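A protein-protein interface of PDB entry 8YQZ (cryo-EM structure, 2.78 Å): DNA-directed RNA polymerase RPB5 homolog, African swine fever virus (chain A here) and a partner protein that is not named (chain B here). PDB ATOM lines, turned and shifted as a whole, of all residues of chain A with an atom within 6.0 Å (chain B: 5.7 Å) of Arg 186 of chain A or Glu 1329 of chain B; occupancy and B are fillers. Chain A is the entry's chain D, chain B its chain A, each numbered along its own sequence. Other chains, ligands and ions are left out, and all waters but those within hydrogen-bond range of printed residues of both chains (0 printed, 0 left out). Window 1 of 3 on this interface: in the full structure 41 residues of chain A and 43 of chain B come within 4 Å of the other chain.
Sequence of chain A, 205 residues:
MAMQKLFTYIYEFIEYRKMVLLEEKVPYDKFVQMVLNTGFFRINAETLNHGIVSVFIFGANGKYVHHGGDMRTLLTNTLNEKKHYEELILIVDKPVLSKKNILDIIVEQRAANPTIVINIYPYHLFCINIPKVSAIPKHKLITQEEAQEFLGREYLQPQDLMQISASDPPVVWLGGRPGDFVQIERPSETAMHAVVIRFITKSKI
The side-chain carboxylate of Glu 857 of chain B is in salt-bridge range of the guanidinium group of Arg 186 of chain A (3.9 Å). OE1 of Glu 857 of chain B is in hydrogen-bond range of OG of Ser 188 of chain A (2.6 Å). The backbone NH (N) of Ile 1328 of chain B lies within hydrogen-bond range of the side-chain carboxylate (OD1) of Asp 168 of chain A, at 3.4 Å. The side-chain carboxylate of Glu 1329 of chain B lies within salt-bridge range of the guanidinium group of Arg 186 of chain A (3.0 Å). The side-chain carboxylate (OE2) of Glu 1329 of chain B lies within salt-bridge range of the guanidinium group (NE) of Arg 198 of chain A, at 3.1 Å. O of Pro 187 of chain A lies within hydrogen-bond range of NE2 of Gln 1333 of chain B, 3.3 Å away. OD2 of Asp 1358 of chain B is in salt-bridge range of NH2 of Arg 186 of chain A.
OE2 of Glu 857 of chain B is in salt-bridge range of NH2 of Arg 1332 of chain B (3.6 Å). The side-chain carboxylate (OD2) of Asp 1358 of chain B is in salt-bridge range of the guanidinium group (NH1) of Arg 1332 of chain B (3.95 Å). ND1 of His 139 of chain A lies within hydrogen-bond range of O of Pro 137 of chain A. O of Val 196 of chain A is in hydrogen-bond range of N of Ile 184 of chain A, at 3.0 Å. The backbone carbonyl oxygen of Ala 194 of chain A lies within hydrogen-bond range of the backbone NH of Arg 186 of chain A (2.9 Å).
CB of Ala 1330 of chain B touches O of Ala 135 of chain A, 3.6 Å away. CB of Glu 1329 of chain B touches CD of Pro 137 of chain A (3.8 Å). His 139 of chain A touches Glu 1329 of chain B. CG1 of Ile 164 of chain A touches CG2 of Ile 1328 of chain B (3.9 Å). OD2 of Asp 168 of chain A touches CA of Gly 1327 of chain B, at 3.4 Å. Glu 1329 of chain B touches Ile 184 of chain A. Arg 186 of chain A touches Arg 1332 of chain B (NH2 to NH1, 3.7 Å). Glu 857 of chain B touches Ala 194 of chain A.
Arg 186 of chain A touches just these residues of chain B: Glu 857, Glu 1329, Arg 1332 and Asp 1358. Printed residues of chain A within 4 Å of Glu 1329 of chain B: Pro 137 (3.8 Å), His 139 (3.9 Å), Ile 184 (3.7 Å), Arg 186 (3.0 Å) and Arg 198 (3.1 Å). Printed residues of chain B within 4 Å of Ser 188 of chain A: Glu 857 (2.6 Å). Of the printed residues of chain B, Ala 135 of chain A touches Ala 1330. Of the printed residues of chain B, Pro 187 of chain A touches Gln 1333 (3.3 Å). The nearest printed residue of chain B that does not touch His 139 of chain A is Ile 1328 of chain B (6.0 Å).
Hydrophobic or aromatic side chains of chain A that line the printed part of chain B: Pro 137, His 139, Ile 164, Ile 184 and Ala 194. Of the 10 printed residues of chain B, 8 touch a printed residue of chain A. Hydrophobic or aromatic side chains of chain B within 4 Å of the printed part of chain A: Ile 1328 and Ala 1330. Among the printed residues, Asp or Glu carboxylates within 4 Å of a Lys or Arg side-chain nitrogen of the other chain: Arg 186 of chain A with Glu 857 of chain B, Arg 186 of chain A with Glu 1329 of chain B, Arg 186 of chain A with Asp 1358 of chain B and Arg 198 of chain A with Glu 1329 of chain B.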
ATOM      1  N   ALA A 135      28.848  19.686 -22.406  1.00  0.00           N
ATOM      2  CA  ALA A 135      29.265  19.911 -21.030  1.00  0.00           C
ATOM      3  C   ALA A 135      29.330  21.378 -20.641  1.00  0.00           C
ATOM      4  O   ALA A 135      29.318  21.677 -19.445  1.00  0.00           O
ATOM      5  CB  ALA A 135      30.632  19.278 -20.797  1.00  0.00           C
ATOM      6  N   PRO A 137      27.908  25.036 -20.138  1.00  0.00           N
ATOM      7  CA  PRO A 137      26.618  25.731 -20.052  1.00  0.00           C
ATOM      8  C   PRO A 137      26.561  26.962 -20.937  1.00  0.00           C
ATOM      9  O   PRO A 137      27.548  27.310 -21.582  1.00  0.00           O
ATOM     10  CB  PRO A 137      26.524  26.110 -18.572  1.00  0.00           C
ATOM     11  CG  PRO A 137      27.538  25.303 -17.892  1.00  0.00           C
ATOM     12  CD  PRO A 137      28.632  25.096 -18.861  1.00  0.00           C
ATOM     13  N   LYS A 138      25.428  27.646 -20.964  1.00  0.00           N
ATOM     14  CA  LYS A 138      25.251  28.804 -21.826  1.00  0.00           C
ATOM     15  C   LYS A 138      25.811  30.046 -21.146  1.00  0.00           C
ATOM     16  O   LYS A 138      25.330  30.450 -20.088  1.00  0.00           O
ATOM     17  CB  LYS A 138      23.778  29.001 -22.160  1.00  0.00           C
ATOM     18  CG  LYS A 138      23.486  28.960 -23.626  1.00  0.00           C
ATOM     19  CD  LYS A 138      23.546  27.525 -24.109  1.00  0.00           C
ATOM     20  CE  LYS A 138      23.761  27.432 -25.601  1.00  0.00           C
ATOM     21  NZ  LYS A 138      24.222  26.080 -25.973  1.00  0.00           N
ATOM     22  N   HIS A 139      26.818  30.651 -21.763  1.00  0.00           N
ATOM     23  CA  HIS A 139      27.424  31.883 -21.295  1.00  0.00           C
ATOM     24  C   HIS A 139      26.887  33.058 -22.097  1.00  0.00           C
ATOM     25  O   HIS A 139      26.556  32.926 -23.272  1.00  0.00           O
ATOM     26  CB  HIS A 139      28.942  31.821 -21.423  1.00  0.00           C
ATOM     27  CG  HIS A 139      29.591  30.814 -20.532  1.00  0.00           C
ATOM     28  ND1 HIS A 139      29.252  29.482 -20.542  1.00  0.00           N
ATOM     29  CD2 HIS A 139      30.596  30.939 -19.638  1.00  0.00           C
ATOM     30  CE1 HIS A 139      29.996  28.835 -19.668  1.00  0.00           C
ATOM     31  NE2 HIS A 139      30.824  29.694 -19.110  1.00  0.00           N
ATOM     32  N   MET A 162      31.804  35.612  -7.893  1.00  0.00           N
ATOM     33  CA  MET A 162      32.711  34.614  -8.430  1.00  0.00           C
ATOM     34  C   MET A 162      33.360  35.153  -9.695  1.00  0.00           C
ATOM     35  O   MET A 162      32.752  35.901 -10.458  1.00  0.00           O
ATOM     36  CB  MET A 162      31.995  33.301  -8.749  1.00  0.00           C
ATOM     37  CG  MET A 162      31.385  32.545  -7.582  1.00  0.00           C
ATOM     38  SD  MET A 162      29.700  32.004  -7.912  1.00  0.00           S
ATOM     39  CE  MET A 162      28.748  33.142  -6.934  1.00  0.00           C
ATOM     40  N   ILE A 164      35.854  34.699 -13.303  1.00  0.00           N
ATOM     41  CA  ILE A 164      36.140  33.829 -14.432  1.00  0.00           C
ATOM     42  C   ILE A 164      37.273  34.455 -15.231  1.00  0.00           C
ATOM     43  O   ILE A 164      37.353  35.680 -15.353  1.00  0.00           O
ATOM     44  CB  ILE A 164      34.882  33.600 -15.296  1.00  0.00           C
ATOM     45  CG1 ILE A 164      35.059  32.396 -16.207  1.00  0.00           C
ATOM     46  CG2 ILE A 164      34.502  34.834 -16.073  1.00  0.00           C
ATOM     47  CD1 ILE A 164      33.789  31.941 -16.803  1.00  0.00           C
ATOM     48  N   ASP A 168      39.020  31.919 -20.583  1.00  0.00           N
ATOM     49  CA  ASP A 168      38.138  30.764 -20.522  1.00  0.00           C
ATOM     50  C   ASP A 168      37.508  30.547 -21.892  1.00  0.00           C
ATOM     51  O   ASP A 168      37.030  31.508 -22.498  1.00  0.00           O
ATOM     52  CB  ASP A 168      37.061  30.996 -19.468  1.00  0.00           C
ATOM     53  CG  ASP A 168      36.671  29.738 -18.737  1.00  0.00           C
ATOM     54  OD1 ASP A 168      37.511  29.193 -17.998  1.00  0.00           O
ATOM     55  OD2 ASP A 168      35.515  29.308 -18.879  1.00  0.00           O
ATOM     56  N   ILE A 184      25.411  32.992 -16.660  1.00  0.00           N
ATOM     57  CA  ILE A 184      25.445  31.589 -17.046  1.00  0.00           C
ATOM     58  C   ILE A 184      24.164  30.911 -16.585  1.00  0.00           C
ATOM     59  O   ILE A 184      23.779  31.032 -15.420  1.00  0.00           O
ATOM     60  CB  ILE A 184      26.684  30.887 -16.465  1.00  0.00           C
ATOM     61  CG1 ILE A 184      27.931  31.690 -16.811  1.00  0.00           C
ATOM     62  CG2 ILE A 184      26.811  29.494 -17.017  1.00  0.00           C
ATOM     63  CD1 ILE A 184      29.082  31.458 -15.918  1.00  0.00           C
ATOM     64  N   GLU A 185      23.513  30.207 -17.502  1.00  0.00           N
ATOM     65  CA  GLU A 185      22.423  29.283 -17.211  1.00  0.00           C
ATOM     66  C   GLU A 185      22.985  27.880 -17.056  1.00  0.00           C
ATOM     67  O   GLU A 185      23.556  27.336 -18.000  1.00  0.00           O
ATOM     68  CB  GLU A 185      21.384  29.310 -18.328  1.00  0.00           C
ATOM     69  CG  GLU A 185      19.993  28.831 -17.941  1.00  0.00           C
ATOM     70  CD  GLU A 185      18.982  29.928 -17.729  1.00  0.00           C
ATOM     71  OE1 GLU A 185      18.423  29.982 -16.614  1.00  0.00           O
ATOM     72  OE2 GLU A 185      18.774  30.751 -18.648  1.00  0.00           O
ATOM     73  N   ARG A 186      22.836  27.296 -15.877  1.00  0.00           N
ATOM     74  CA  ARG A 186      23.444  25.988 -15.740  1.00  0.00           C
ATOM     75  C   ARG A 186      22.452  24.952 -15.240  1.00  0.00           C
ATOM     76  O   ARG A 186      21.562  25.260 -14.449  1.00  0.00           O
ATOM     77  CB  ARG A 186      24.671  26.037 -14.820  1.00  0.00           C
ATOM     78  CG  ARG A 186      24.467  26.425 -13.397  1.00  0.00           C
ATOM     79  CD  ARG A 186      25.735  27.087 -12.925  1.00  0.00           C
ATOM     80  NE  ARG A 186      25.791  27.257 -11.482  1.00  0.00           N
ATOM     81  CZ  ARG A 186      26.873  27.630 -10.815  1.00  0.00           C
ATOM     82  NH1 ARG A 186      28.002  27.916 -11.432  1.00  0.00           N
ATOM     83  NH2 ARG A 186      26.817  27.723  -9.497  1.00  0.00           N
ATOM     84  N   PRO A 187      22.581  23.715 -15.712  1.00  0.00           N
ATOM     85  CA  PRO A 187      21.668  22.654 -15.283  1.00  0.00           C
ATOM     86  C   PRO A 187      21.851  22.316 -13.817  1.00  0.00           C
ATOM     87  O   PRO A 187      22.965  22.312 -13.294  1.00  0.00           O
ATOM     88  CB  PRO A 187      22.063  21.471 -16.171  1.00  0.00           C
ATOM     89  CG  PRO A 187      22.894  22.044 -17.232  1.00  0.00           C
ATOM     90  CD  PRO A 187      23.571  23.215 -16.668  1.00  0.00           C
ATOM     91  N   SER A 188      20.750  21.993 -13.163  1.00  0.00           N
ATOM     92  CA  SER A 188      20.763  21.721 -11.740  1.00  0.00           C
ATOM     93  C   SER A 188      20.022  20.422 -11.483  1.00  0.00           C
ATOM     94  O   SER A 188      18.970  20.179 -12.073  1.00  0.00           O
ATOM     95  CB  SER A 188      20.129  22.883 -10.962  1.00  0.00           C
ATOM     96  OG  SER A 188      20.394  22.785  -9.582  1.00  0.00           O
ATOM     97  N   MET A 192      16.462  22.132 -11.321  1.00  0.00           N
ATOM     98  CA  MET A 192      16.366  21.930 -12.765  1.00  0.00           C
ATOM     99  C   MET A 192      17.102  22.981 -13.593  1.00  0.00           C
ATOM    100  O   MET A 192      17.490  22.688 -14.721  1.00  0.00           O
ATOM    101  CB  MET A 192      14.900  21.892 -13.205  1.00  0.00           C
ATOM    102  CG  MET A 192      14.671  21.417 -14.626  1.00  0.00           C
ATOM    103  SD  MET A 192      13.514  22.431 -15.546  1.00  0.00           S
ATOM    104  CE  MET A 192      12.007  22.123 -14.658  1.00  0.00           C
ATOM    105  N   HIS A 193      17.408  24.146 -13.021  1.00  0.00           N
ATOM    106  CA  HIS A 193      18.330  25.106 -13.625  1.00  0.00           C
ATOM    107  C   HIS A 193      18.548  26.317 -12.730  1.00  0.00           C
ATOM    108  O   HIS A 193      17.684  26.667 -11.927  1.00  0.00           O
ATOM    109  CB  HIS A 193      17.880  25.552 -15.024  1.00  0.00           C
ATOM    110  CG  HIS A 193      16.472  26.044 -15.110  1.00  0.00           C
ATOM    111  ND1 HIS A 193      15.916  26.454 -16.298  1.00  0.00           N
ATOM    112  CD2 HIS A 193      15.517  26.210 -14.171  1.00  0.00           C
ATOM    113  CE1 HIS A 193      14.675  26.842 -16.089  1.00  0.00           C
ATOM    114  NE2 HIS A 193      14.408  26.704 -14.806  1.00  0.00           N
ATOM    115  N   ALA A 194      19.697  26.968 -12.882  1.00  0.00           N
ATOM    116  CA  ALA A 194      20.134  28.045 -12.009  1.00  0.00           C
ATOM    117  C   ALA A 194      20.799  29.119 -12.851  1.00  0.00           C
ATOM    118  O   ALA A 194      21.225  28.871 -13.974  1.00  0.00           O
ATOM    119  CB  ALA A 194      21.101  27.530 -10.944  1.00  0.00           C
ATOM    120  N   VAL A 195      20.874  30.329 -12.313  1.00  0.00           N
ATOM    121  CA  VAL A 195      21.548  31.440 -12.975  1.00  0.00           C
ATOM    122  C   VAL A 195      22.586  32.020 -12.023  1.00  0.00           C
ATOM    123  O   VAL A 195      22.281  32.289 -10.858  1.00  0.00           O
ATOM    124  CB  VAL A 195      20.549  32.521 -13.420  1.00  0.00           C
ATOM    125  CG1 VAL A 195      21.272  33.776 -13.813  1.00  0.00           C
ATOM    126  CG2 VAL A 195      19.738  32.046 -14.576  1.00  0.00           C
ATOM    127  N   VAL A 196      23.816  32.186 -12.510  1.00  0.00           N
ATOM    128  CA  VAL A 196      24.871  32.871 -11.778  1.00  0.00           C
ATOM    129  C   VAL A 196      25.441  33.964 -12.666  1.00  0.00           C
ATOM    130  O   VAL A 196      25.247  33.976 -13.877  1.00  0.00           O
ATOM    131  CB  VAL A 196      25.992  31.926 -11.303  1.00  0.00           C
ATOM    132  CG1 VAL A 196      25.452  30.925 -10.319  1.00  0.00           C
ATOM    133  CG2 VAL A 196      26.644  31.244 -12.472  1.00  0.00           C
ATOM    134  N   ARG A 198      29.177  35.972 -13.156  1.00  0.00           N
ATOM    135  CA  ARG A 198      30.593  35.943 -12.847  1.00  0.00           C
ATOM    136  C   ARG A 198      31.258  37.216 -13.348  1.00  0.00           C
ATOM    137  O   ARG A 198      30.744  37.907 -14.222  1.00  0.00           O
ATOM    138  CB  ARG A 198      31.267  34.723 -13.467  1.00  0.00           C
ATOM    139  CG  ARG A 198      31.030  33.453 -12.712  1.00  0.00           C
ATOM    140  CD  ARG A 198      31.882  32.344 -13.225  1.00  0.00           C
ATOM    141  NE  ARG A 198      31.807  31.176 -12.363  1.00  0.00           N
ATOM    142  CZ  ARG A 198      32.754  30.800 -11.520  1.00  0.00           C
ATOM    143  NH1 ARG A 198      33.894  31.449 -11.429  1.00  0.00           N
ATOM    144  NH2 ARG A 198      32.558  29.731 -10.764  1.00  0.00           N
ATOM    145  N   GLU B 857      21.147  25.906  -4.807  1.00  0.00           N
ATOM    146  CA  GLU B 857      20.461  26.392  -5.999  1.00  0.00           C
ATOM    147  C   GLU B 857      18.954  26.428  -5.847  1.00  0.00           C
ATOM    148  O   GLU B 857      18.260  26.907  -6.742  1.00  0.00           O
ATOM    149  CB  GLU B 857      20.842  25.569  -7.218  1.00  0.00           C
ATOM    150  CG  GLU B 857      22.205  25.901  -7.719  1.00  0.00           C
ATOM    151  CD  GLU B 857      22.903  24.724  -8.301  1.00  0.00           C
ATOM    152  OE1 GLU B 857      22.370  23.606  -8.185  1.00  0.00           O
ATOM    153  OE2 GLU B 857      23.992  24.916  -8.870  1.00  0.00           O
ATOM    154  N   GLY B1327      36.651  24.854 -19.622  1.00  0.00           N
ATOM    155  CA  GLY B1327      36.486  26.027 -18.799  1.00  0.00           C
ATOM    156  C   GLY B1327      36.149  25.659 -17.377  1.00  0.00           C
ATOM    157  O   GLY B1327      36.209  24.494 -16.979  1.00  0.00           O
ATOM    158  N   ILE B1328      35.771  26.669 -16.596  1.00  0.00           N
ATOM    159  CA  ILE B1328      35.568  26.461 -15.166  1.00  0.00           C
ATOM    160  C   ILE B1328      34.194  25.885 -14.872  1.00  0.00           C
ATOM    161  O   ILE B1328      34.048  25.071 -13.960  1.00  0.00           O
ATOM    162  CB  ILE B1328      35.818  27.769 -14.389  1.00  0.00           C
ATOM    163  CG1 ILE B1328      35.847  27.498 -12.892  1.00  0.00           C
ATOM    164  CG2 ILE B1328      34.784  28.822 -14.705  1.00  0.00           C
ATOM    165  CD1 ILE B1328      36.907  26.549 -12.490  1.00  0.00           C
ATOM    166  N   GLU B1329      33.170  26.278 -15.625  1.00  0.00           N
ATOM    167  CA  GLU B1329      31.822  25.822 -15.329  1.00  0.00           C
ATOM    168  C   GLU B1329      31.648  24.345 -15.633  1.00  0.00           C
ATOM    169  O   GLU B1329      30.901  23.654 -14.935  1.00  0.00           O
ATOM    170  CB  GLU B1329      30.818  26.658 -16.106  1.00  0.00           C
ATOM    171  CG  GLU B1329      30.610  28.045 -15.535  1.00  0.00           C
ATOM    172  CD  GLU B1329      29.744  28.047 -14.302  1.00  0.00           C
ATOM    173  OE1 GLU B1329      28.798  27.241 -14.239  1.00  0.00           O
ATOM    174  OE2 GLU B1329      30.006  28.849 -13.389  1.00  0.00           O
ATOM    175  N   ALA B1330      32.311  23.846 -16.671  1.00  0.00           N
ATOM    176  CA  ALA B1330      32.273  22.420 -16.955  1.00  0.00           C
ATOM    177  C   ALA B1330      33.125  21.633 -15.975  1.00  0.00           C
ATOM    178  O   ALA B1330      32.791  20.494 -15.646  1.00  0.00           O
ATOM    179  CB  ALA B1330      32.730  22.168 -18.386  1.00  0.00           C
ATOM    180  N   ALA B1331      34.225  22.219 -15.503  1.00  0.00           N
ATOM    181  CA  ALA B1331      35.044  21.572 -14.487  1.00  0.00           C
ATOM    182  C   ALA B1331      34.331  21.494 -13.143  1.00  0.00           C
ATOM    183  O   ALA B1331      34.608  20.591 -12.353  1.00  0.00           O
ATOM    184  CB  ALA B1331      36.367  22.310 -14.340  1.00  0.00           C
ATOM    185  N   ARG B1332      33.431  22.432 -12.854  1.00  0.00           N
ATOM    186  CA  ARG B1332      32.622  22.333 -11.647  1.00  0.00           C
ATOM    187  C   ARG B1332      31.647  21.169 -11.724  1.00  0.00           C
ATOM    188  O   ARG B1332      31.506  20.412 -10.761  1.00  0.00           O
ATOM    189  CB  ARG B1332      31.872  23.636 -11.411  1.00  0.00           C
ATOM    190  CG  ARG B1332      31.158  23.693 -10.087  1.00  0.00           C
ATOM    191  CD  ARG B1332      30.126  24.772 -10.077  1.00  0.00           C
ATOM    192  NE  ARG B1332      28.905  24.351 -10.746  1.00  0.00           N
ATOM    193  CZ  ARG B1332      27.764  24.076 -10.131  1.00  0.00           C
ATOM    194  NH1 ARG B1332      27.642  24.182  -8.821  1.00  0.00           N
ATOM    195  NH2 ARG B1332      26.716  23.702 -10.852  1.00  0.00           N
ATOM    196  N   GLN B1333      30.960  21.010 -12.854  1.00  0.00           N
ATOM    197  CA  GLN B1333      30.099  19.850 -13.044  1.00  0.00           C
ATOM    198  C   GLN B1333      30.885  18.553 -12.972  1.00  0.00           C
ATOM    199  O   GLN B1333      30.360  17.543 -12.508  1.00  0.00           O
ATOM    200  CB  GLN B1333      29.383  19.930 -14.384  1.00  0.00           C
ATOM    201  CG  GLN B1333      28.314  20.972 -14.493  1.00  0.00           C
ATOM    202  CD  GLN B1333      27.072  20.639 -13.708  1.00  0.00           C
ATOM    203  OE1 GLN B1333      26.933  19.546 -13.173  1.00  0.00           O
ATOM    204  NE2 GLN B1333      26.140  21.573 -13.670  1.00  0.00           N
ATOM    205  N   LYS B1334      32.127  18.561 -13.443  1.00  0.00           N
ATOM    206  CA  LYS B1334      32.965  17.372 -13.378  1.00  0.00           C
ATOM    207  C   LYS B1334      33.267  16.971 -11.943  1.00  0.00           C
ATOM    208  O   LYS B1334      33.293  15.781 -11.625  1.00  0.00           O
ATOM    209  CB  LYS B1334      34.258  17.610 -14.160  1.00  0.00           C
ATOM    210  CG  LYS B1334      35.176  16.407 -14.278  1.00  0.00           C
ATOM    211  CD  LYS B1334      34.454  15.172 -14.764  1.00  0.00           C
ATOM    212  CE  LYS B1334      33.886  15.366 -16.140  1.00  0.00           C
ATOM    213  NZ  LYS B1334      33.097  14.189 -16.569  1.00  0.00           N
ATOM    214  N   ASP B1358      31.365  24.271  -5.645  1.00  0.00           N
ATOM    215  CA  ASP B1358      31.296  25.719  -5.767  1.00  0.00           C
ATOM    216  C   ASP B1358      32.383  26.417  -4.966  1.00  0.00           C
ATOM    217  O   ASP B1358      32.771  27.536  -5.302  1.00  0.00           O
ATOM    218  CB  ASP B1358      29.919  26.205  -5.338  1.00  0.00           C
ATOM    219  CG  ASP B1358      28.971  26.358  -6.504  1.00  0.00           C
ATOM    220  OD1 ASP B1358      28.387  25.355  -6.936  1.00  0.00           O
ATOM    221  OD2 ASP B1358      28.791  27.488  -6.984  1.00  0.00           O
